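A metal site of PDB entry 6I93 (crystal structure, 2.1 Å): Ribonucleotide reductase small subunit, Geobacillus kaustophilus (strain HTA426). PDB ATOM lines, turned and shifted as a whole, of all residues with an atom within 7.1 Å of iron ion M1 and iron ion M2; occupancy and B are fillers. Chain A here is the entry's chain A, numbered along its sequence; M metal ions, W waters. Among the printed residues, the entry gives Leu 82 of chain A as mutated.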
ATOM      1  N   PHE A  79      -6.199 -12.995  -5.045  1.00  0.00           N
ATOM      2  CA  PHE A  79      -4.999 -12.459  -5.665  1.00  0.00           C
ATOM      3  C   PHE A  79      -4.081 -11.808  -4.650  1.00  0.00           C
ATOM      4  O   PHE A  79      -2.863 -12.008  -4.716  1.00  0.00           O
ATOM      5  CB  PHE A  79      -5.366 -11.464  -6.734  1.00  0.00           C
ATOM      6  CG  PHE A  79      -5.203 -11.980  -8.121  1.00  0.00           C
ATOM      7  CD1 PHE A  79      -3.923 -12.143  -8.665  1.00  0.00           C
ATOM      8  CD2 PHE A  79      -6.322 -12.296  -8.903  1.00  0.00           C
ATOM      9  CE1 PHE A  79      -3.771 -12.640  -9.979  1.00  0.00           C
ATOM     10  CE2 PHE A  79      -6.169 -12.771 -10.207  1.00  0.00           C
ATOM     11  CZ  PHE A  79      -4.887 -12.941 -10.744  1.00  0.00           C
ATOM     12  N   LEU A  82      -2.263 -14.350  -3.090  1.00  0.00           N
ATOM     13  CA  LEU A  82      -1.354 -14.932  -4.070  1.00  0.00           C
ATOM     14  C   LEU A  82      -0.072 -14.119  -4.174  1.00  0.00           C
ATOM     15  O   LEU A  82       1.035 -14.651  -4.071  1.00  0.00           O
ATOM     16  CB  LEU A  82      -2.021 -15.036  -5.460  1.00  0.00           C
ATOM     17  CG  LEU A  82      -1.265 -15.759  -6.615  1.00  0.00           C
ATOM     18  CD1 LEU A  82      -2.292 -16.344  -7.602  1.00  0.00           C
ATOM     19  CD2 LEU A  82      -0.270 -14.919  -7.403  1.00  0.00           C
ATOM     20  N   GLU A  83      -0.215 -12.810  -4.420  1.00  0.00           N
ATOM     21  CA  GLU A  83       0.957 -11.956  -4.588  1.00  0.00           C
ATOM     22  C   GLU A  83       1.805 -11.938  -3.317  1.00  0.00           C
ATOM     23  O   GLU A  83       3.042 -12.026  -3.380  1.00  0.00           O
ATOM     24  CB  GLU A  83       0.531 -10.548  -4.975  1.00  0.00           C
ATOM     25  CG  GLU A  83      -0.407 -10.452  -6.150  1.00  0.00           C
ATOM     26  CD  GLU A  83       0.129 -11.070  -7.423  1.00  0.00           C
ATOM     27  OE1 GLU A  83      -0.686 -11.386  -8.317  1.00  0.00           O
ATOM     28  OE2 GLU A  83       1.367 -11.196  -7.548  1.00  0.00           O
ATOM     29  N   VAL A  86       3.727 -15.370  -2.927  1.00  0.00           N
ATOM     30  CA  VAL A  86       4.841 -15.565  -3.862  1.00  0.00           C
ATOM     31  C   VAL A  86       5.960 -14.533  -3.614  1.00  0.00           C
ATOM     32  O   VAL A  86       7.135 -14.844  -3.864  1.00  0.00           O
ATOM     33  CB  VAL A  86       4.332 -15.530  -5.331  1.00  0.00           C
ATOM     34  CG1 VAL A  86       3.304 -16.674  -5.594  1.00  0.00           C
ATOM     35  CG2 VAL A  86       3.776 -14.183  -5.709  1.00  0.00           C
ATOM     36  N   THR A  87       5.657 -13.331  -3.109  1.00  0.00           N
ATOM     37  CA  THR A  87       6.734 -12.423  -2.714  1.00  0.00           C
ATOM     38  C   THR A  87       7.613 -13.068  -1.627  1.00  0.00           C
ATOM     39  O   THR A  87       8.848 -13.106  -1.740  1.00  0.00           O
ATOM     40  CB  THR A  87       6.194 -11.058  -2.220  1.00  0.00           C
ATOM     41  OG1 THR A  87       5.370 -10.425  -3.208  1.00  0.00           O
ATOM     42  CG2 THR A  87       7.386 -10.087  -1.922  1.00  0.00           C
ATOM     43  N   PHE A 112      12.290 -10.786 -10.389  1.00  0.00           N
ATOM     44  CA  PHE A 112      11.121 -11.564 -10.067  1.00  0.00           C
ATOM     45  C   PHE A 112      10.548 -11.125  -8.713  1.00  0.00           C
ATOM     46  O   PHE A 112       9.381 -10.777  -8.609  1.00  0.00           O
ATOM     47  CB  PHE A 112      11.545 -13.047 -10.054  1.00  0.00           C
ATOM     48  CG  PHE A 112      10.407 -14.076 -10.072  1.00  0.00           C
ATOM     49  CD1 PHE A 112      10.533 -15.231 -10.839  1.00  0.00           C
ATOM     50  CD2 PHE A 112       9.281 -13.925  -9.299  1.00  0.00           C
ATOM     51  CE1 PHE A 112       9.546 -16.196 -10.852  1.00  0.00           C
ATOM     52  CE2 PHE A 112       8.269 -14.899  -9.331  1.00  0.00           C
ATOM     53  CZ  PHE A 112       8.400 -16.026 -10.081  1.00  0.00           C
ATOM     54  N   ASP A 115       9.099  -7.657  -8.881  1.00  0.00           N
ATOM     55  CA  ASP A 115       7.804  -7.668  -9.538  1.00  0.00           C
ATOM     56  C   ASP A 115       6.720  -8.040  -8.532  1.00  0.00           C
ATOM     57  O   ASP A 115       5.640  -7.432  -8.503  1.00  0.00           O
ATOM     58  CB  ASP A 115       7.779  -8.677 -10.691  1.00  0.00           C
ATOM     59  CG  ASP A 115       8.631  -8.264 -11.889  1.00  0.00           C
ATOM     60  OD1 ASP A 115       8.968  -7.111 -11.973  1.00  0.00           O
ATOM     61  OD2 ASP A 115       8.920  -9.078 -12.780  1.00  0.00           O
ATOM     62  N   GLU A 116       6.960  -9.083  -7.739  1.00  0.00           N
ATOM     63  CA  GLU A 116       5.910  -9.593  -6.874  1.00  0.00           C
ATOM     64  C   GLU A 116       5.592  -8.576  -5.781  1.00  0.00           C
ATOM     65  O   GLU A 116       4.422  -8.359  -5.439  1.00  0.00           O
ATOM     66  CB  GLU A 116       6.319 -10.947  -6.277  1.00  0.00           C
ATOM     67  CG  GLU A 116       6.621 -12.095  -7.255  1.00  0.00           C
ATOM     68  CD  GLU A 116       5.432 -12.426  -8.211  1.00  0.00           C
ATOM     69  OE1 GLU A 116       5.507 -13.407  -8.946  1.00  0.00           O
ATOM     70  OE2 GLU A 116       4.401 -11.750  -8.193  1.00  0.00           O
ATOM     71  N   ALA A 117       6.610  -7.855  -5.277  1.00  0.00           N
ATOM     72  CA  ALA A 117       6.366  -6.773  -4.331  1.00  0.00           C
ATOM     73  C   ALA A 117       5.443  -5.710  -4.937  1.00  0.00           C
ATOM     74  O   ALA A 117       4.520  -5.228  -4.278  1.00  0.00           O
ATOM     75  CB  ALA A 117       7.688  -6.154  -3.871  1.00  0.00           C
ATOM     76  N   HIS A 119       3.294  -6.337  -7.184  1.00  0.00           N
ATOM     77  CA  HIS A 119       1.954  -6.923  -7.346  1.00  0.00           C
ATOM     78  C   HIS A 119       1.158  -6.829  -6.047  1.00  0.00           C
ATOM     79  O   HIS A 119      -0.016  -6.452  -6.050  1.00  0.00           O
ATOM     80  CB  HIS A 119       2.042  -8.360  -7.825  1.00  0.00           C
ATOM     81  CG  HIS A 119       2.677  -8.465  -9.190  1.00  0.00           C
ATOM     82  ND1 HIS A 119       2.930  -9.672  -9.798  1.00  0.00           N
ATOM     83  CD2 HIS A 119       3.127  -7.507 -10.026  1.00  0.00           C
ATOM     84  CE1 HIS A 119       3.509  -9.450 -10.964  1.00  0.00           C
ATOM     85  NE2 HIS A 119       3.654  -8.140 -11.126  1.00  0.00           N
ATOM     86  N   VAL A 120       1.798  -7.156  -4.929  1.00  0.00           N
ATOM     87  CA  VAL A 120       1.202  -6.996  -3.603  1.00  0.00           C
ATOM     88  C   VAL A 120       0.732  -5.584  -3.419  1.00  0.00           C
ATOM     89  O   VAL A 120      -0.338  -5.336  -2.861  1.00  0.00           O
ATOM     90  CB  VAL A 120       2.225  -7.320  -2.502  1.00  0.00           C
ATOM     91  CG1 VAL A 120       1.638  -6.949  -1.099  1.00  0.00           C
ATOM     92  CG2 VAL A 120       2.523  -8.742  -2.510  1.00  0.00           C
ATOM     93  N   PHE A 123      -2.521  -4.491  -5.549  1.00  0.00           N
ATOM     94  CA  PHE A 123      -3.829  -4.884  -5.015  1.00  0.00           C
ATOM     95  C   PHE A 123      -4.137  -4.171  -3.703  1.00  0.00           C
ATOM     96  O   PHE A 123      -5.284  -3.802  -3.453  1.00  0.00           O
ATOM     97  CB  PHE A 123      -3.913  -6.391  -4.821  1.00  0.00           C
ATOM     98  CG  PHE A 123      -4.087  -7.169  -6.133  1.00  0.00           C
ATOM     99  CD1 PHE A 123      -5.258  -7.069  -6.894  1.00  0.00           C
ATOM    100  CD2 PHE A 123      -3.076  -7.991  -6.605  1.00  0.00           C
ATOM    101  CE1 PHE A 123      -5.408  -7.770  -8.121  1.00  0.00           C
ATOM    102  CE2 PHE A 123      -3.211  -8.696  -7.825  1.00  0.00           C
ATOM    103  CZ  PHE A 123      -4.370  -8.584  -8.591  1.00  0.00           C
ATOM    104  N   TYR A 176       4.798 -23.347  -7.991  1.00  0.00           N
ATOM    105  CA  TYR A 176       4.853 -21.886  -8.012  1.00  0.00           C
ATOM    106  C   TYR A 176       4.619 -21.329  -9.419  1.00  0.00           C
ATOM    107  O   TYR A 176       3.699 -20.541  -9.628  1.00  0.00           O
ATOM    108  CB  TYR A 176       6.217 -21.436  -7.481  1.00  0.00           C
ATOM    109  CG  TYR A 176       6.382 -19.974  -7.214  1.00  0.00           C
ATOM    110  CD1 TYR A 176       6.862 -19.555  -5.984  1.00  0.00           C
ATOM    111  CD2 TYR A 176       6.152 -19.026  -8.169  1.00  0.00           C
ATOM    112  CE1 TYR A 176       7.056 -18.225  -5.707  1.00  0.00           C
ATOM    113  CE2 TYR A 176       6.356 -17.676  -7.904  1.00  0.00           C
ATOM    114  CZ  TYR A 176       6.814 -17.288  -6.657  1.00  0.00           C
ATOM    115  OH  TYR A 176       7.013 -15.951  -6.374  1.00  0.00           O
ATOM    116  N   ASN A 177       5.455 -21.731 -10.386  1.00  0.00           N
ATOM    117  CA  ASN A 177       5.443 -21.074 -11.684  1.00  0.00           C
ATOM    118  C   ASN A 177       4.398 -21.661 -12.621  1.00  0.00           C
ATOM    119  O   ASN A 177       3.771 -20.920 -13.404  1.00  0.00           O
ATOM    120  CB  ASN A 177       6.818 -21.177 -12.338  1.00  0.00           C
ATOM    121  CG  ASN A 177       7.936 -20.683 -11.438  1.00  0.00           C
ATOM    122  OD1 ASN A 177       8.797 -21.443 -11.038  1.00  0.00           O
ATOM    123  ND2 ASN A 177       7.896 -19.407 -11.086  1.00  0.00           N
ATOM    124  N   VAL A 180       0.542 -22.031  -9.579  1.00  0.00           N
ATOM    125  CA  VAL A 180       0.065 -20.782  -8.987  1.00  0.00           C
ATOM    126  C   VAL A 180       0.062 -19.654 -10.024  1.00  0.00           C
ATOM    127  O   VAL A 180      -0.927 -18.926 -10.161  1.00  0.00           O
ATOM    128  CB  VAL A 180       0.918 -20.437  -7.737  1.00  0.00           C
ATOM    129  CG1 VAL A 180       0.867 -18.961  -7.397  1.00  0.00           C
ATOM    130  CG2 VAL A 180       0.421 -21.249  -6.541  1.00  0.00           C
ATOM    131  N   GLU A 181       1.163 -19.490 -10.762  1.00  0.00           N
ATOM    132  CA  GLU A 181       1.263 -18.424 -11.758  1.00  0.00           C
ATOM    133  C   GLU A 181       0.682 -18.900 -13.093  1.00  0.00           C
ATOM    134  O   GLU A 181      -0.250 -18.293 -13.642  1.00  0.00           O
ATOM    135  CB  GLU A 181       2.741 -18.007 -11.912  1.00  0.00           C
ATOM    136  CG  GLU A 181       3.397 -17.290 -10.704  1.00  0.00           C
ATOM    137  CD  GLU A 181       4.881 -17.037 -10.913  1.00  0.00           C
ATOM    138  OE1 GLU A 181       5.606 -17.938 -11.389  1.00  0.00           O
ATOM    139  OE2 GLU A 181       5.321 -15.915 -10.586  1.00  0.00           O
ATOM    140  N   ALA A 185      -3.048 -17.708 -11.661  1.00  0.00           N
ATOM    141  CA  ALA A 185      -2.943 -16.265 -11.890  1.00  0.00           C
ATOM    142  C   ALA A 185      -3.389 -15.916 -13.318  1.00  0.00           C
ATOM    143  O   ALA A 185      -4.135 -14.962 -13.531  1.00  0.00           O
ATOM    144  CB  ALA A 185      -1.528 -15.785 -11.653  1.00  0.00           C
ATOM    145  N   TYR A 189      -6.301 -13.330 -14.510  1.00  0.00           N
ATOM    146  CA  TYR A 189      -6.175 -12.158 -15.368  1.00  0.00           C
ATOM    147  C   TYR A 189      -7.271 -12.187 -16.430  1.00  0.00           C
ATOM    148  O   TYR A 189      -7.957 -11.182 -16.646  1.00  0.00           O
ATOM    149  CB  TYR A 189      -4.812 -12.098 -16.078  1.00  0.00           C
ATOM    150  CG  TYR A 189      -3.585 -12.115 -15.200  1.00  0.00           C
ATOM    151  CD1 TYR A 189      -3.594 -11.503 -13.960  1.00  0.00           C
ATOM    152  CD2 TYR A 189      -2.414 -12.764 -15.602  1.00  0.00           C
ATOM    153  CE1 TYR A 189      -2.503 -11.516 -13.153  1.00  0.00           C
ATOM    154  CE2 TYR A 189      -1.289 -12.793 -14.791  1.00  0.00           C
ATOM    155  CZ  TYR A 189      -1.356 -12.160 -13.557  1.00  0.00           C
ATOM    156  OH  TYR A 189      -0.308 -12.138 -12.697  1.00  0.00           O
ATOM    157  N   LEU A 212       0.684  -6.683 -14.444  1.00  0.00           N
ATOM    158  CA  LEU A 212       0.974  -7.969 -13.797  1.00  0.00           C
ATOM    159  C   LEU A 212       1.113  -9.069 -14.833  1.00  0.00           C
ATOM    160  O   LEU A 212       2.030  -9.889 -14.756  1.00  0.00           O
ATOM    161  CB  LEU A 212      -0.132  -8.365 -12.798  1.00  0.00           C
ATOM    162  CG  LEU A 212       0.029  -8.033 -11.320  1.00  0.00           C
ATOM    163  CD1 LEU A 212       0.332  -6.565 -11.144  1.00  0.00           C
ATOM    164  CD2 LEU A 212      -1.206  -8.418 -10.605  1.00  0.00           C
ATOM    165  N   ASP A 215       4.494  -8.928 -16.507  1.00  0.00           N
ATOM    166  CA  ASP A 215       5.518  -9.477 -15.645  1.00  0.00           C
ATOM    167  C   ASP A 215       5.415 -11.006 -15.614  1.00  0.00           C
ATOM    168  O   ASP A 215       6.441 -11.689 -15.638  1.00  0.00           O
ATOM    169  CB  ASP A 215       5.403  -8.906 -14.221  1.00  0.00           C
ATOM    170  CG  ASP A 215       5.504  -7.404 -14.141  1.00  0.00           C
ATOM    171  OD1 ASP A 215       6.202  -6.773 -14.991  1.00  0.00           O
ATOM    172  OD2 ASP A 215       4.923  -6.855 -13.175  1.00  0.00           O
ATOM    173  N   GLU A 216       4.194 -11.544 -15.576  1.00  0.00           N
ATOM    174  CA  GLU A 216       4.004 -12.979 -15.330  1.00  0.00           C
ATOM    175  C   GLU A 216       4.620 -13.824 -16.423  1.00  0.00           C
ATOM    176  O   GLU A 216       5.031 -14.961 -16.167  1.00  0.00           O
ATOM    177  CB  GLU A 216       2.523 -13.323 -15.215  1.00  0.00           C
ATOM    178  CG  GLU A 216       2.202 -14.638 -14.460  1.00  0.00           C
ATOM    179  CD  GLU A 216       2.468 -14.493 -12.980  1.00  0.00           C
ATOM    180  OE1 GLU A 216       1.534 -14.187 -12.198  1.00  0.00           O
ATOM    181  OE2 GLU A 216       3.638 -14.670 -12.610  1.00  0.00           O
ATOM    182  N   GLY A 217       4.641 -13.306 -17.642  1.00  0.00           N
ATOM    183  CA  GLY A 217       5.324 -13.993 -18.736  1.00  0.00           C
ATOM    184  C   GLY A 217       6.765 -14.358 -18.426  1.00  0.00           C
ATOM    185  O   GLY A 217       7.183 -15.481 -18.692  1.00  0.00           O
ATOM    186  N   HIS A 219       7.995 -14.699 -15.343  1.00  0.00           N
ATOM    187  CA  HIS A 219       7.966 -15.634 -14.226  1.00  0.00           C
ATOM    188  C   HIS A 219       7.770 -17.050 -14.731  1.00  0.00           C
ATOM    189  O   HIS A 219       8.528 -17.953 -14.380  1.00  0.00           O
ATOM    190  CB  HIS A 219       6.851 -15.232 -13.250  1.00  0.00           C
ATOM    191  CG  HIS A 219       6.994 -13.846 -12.719  1.00  0.00           C
ATOM    192  ND1 HIS A 219       6.122 -13.297 -11.803  1.00  0.00           N
ATOM    193  CD2 HIS A 219       7.910 -12.891 -12.985  1.00  0.00           C
ATOM    194  CE1 HIS A 219       6.483 -12.061 -11.541  1.00  0.00           C
ATOM    195  NE2 HIS A 219       7.563 -11.782 -12.247  1.00  0.00           N
ATOM    196  N   ILE A 220       6.808 -17.234 -15.633  1.00  0.00           N
ATOM    197  CA  ILE A 220       6.533 -18.537 -16.203  1.00  0.00           C
ATOM    198  C   ILE A 220       7.718 -19.040 -17.035  1.00  0.00           C
ATOM    199  O   ILE A 220       8.037 -20.226 -17.035  1.00  0.00           O
ATOM    200  CB  ILE A 220       5.210 -18.456 -17.012  1.00  0.00           C
ATOM    201  CG1 ILE A 220       4.034 -18.149 -16.054  1.00  0.00           C
ATOM    202  CG2 ILE A 220       4.977 -19.775 -17.786  1.00  0.00           C
ATOM    203  CD1 ILE A 220       2.670 -17.681 -16.705  1.00  0.00           C
HETATM  204 FE    FE M   1       2.416 -11.738  -9.244  1.00  0.00          FE
HETATM  205 FE    FE M   2       4.457 -14.050 -10.675  1.00  0.00          FE
HETATM  206  O   HOH W   1       0.273 -11.938 -10.443  1.00  0.00           O
HETATM  207  O   HOH W   2       3.433 -12.355 -11.037  1.00  0.00           O
HETATM  208  O   HOH W   3       2.517 -14.012  -9.430  1.00  0.00           O
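The backbone NH of Glu 181 is in hydrogen-bond range of the backbone carbonyl oxygen of Tyr 176, at 3.0 Å. OE1 of Glu 181 lies within hydrogen-bond range of ND2 of Asn 177. The backbone carbonyl oxygen of Glu 83 lies within hydrogen-bond range of the side-chain hydroxyl of Thr 87. The side-chain hydroxyl of Thr 87 lies close to the backbone carbonyl oxygen of Glu 116 (3.2 Å). The side-chain carboxylate (OD2) of Asp 115 sits at hydrogen-bond distance from a ring nitrogen (NE2) of His 219 (3.1 Å). The side-chain carboxylate (OE1) of Glu 216 lies within hydrogen-bond range of the side-chain hydroxyl (OH) of Tyr 189 (2.8 Å). A ring nitrogen (NE2) of His 119 lies close to the backbone carbonyl oxygen of Asp 115. The side-chain carboxylate (OD2) of Asp 215 is in hydrogen-bond range of a ring nitrogen (NE2) of His 119, at 2.7 Å.
Of the 24 residues printed, 4 come within 4 Å of iron ion M1. Along chain A the residues within 4 Å of iron ion M1 span positions 83 to 216. The nearest printed residue that does not touch iron ion M1 is Tyr 189 (4.4 Å).
Iron ion M2 is bound by water W2 (2.0 Å), the side-chain carboxylate (OE2) of Glu 181 (2.1 Å), the side-chain carboxylate (OE1) of Glu 116 (2.1 Å), a ring nitrogen (ND1) of His 219 (2.1 Å), the side-chain carboxylate (OE2) of Glu 216 (2.2 Å) and water W3 (2.3 Å). Iron ion M2 has six donor atoms within binding distance.
Iron ion M1 is bound by the side-chain carboxylate of Glu 83 (2.1 Å), water W2 (2.2 Å), a ring nitrogen (ND1) of His 119 (2.2 Å), the side-chain carboxylate of Glu 116 (2.2 Å), water W3 (2.3 Å) and water W1 (2.5 Å).
Four residues have an atom within 4 Å of iron ion M2: Glu 116, Glu 181, Glu 216 and His 219.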
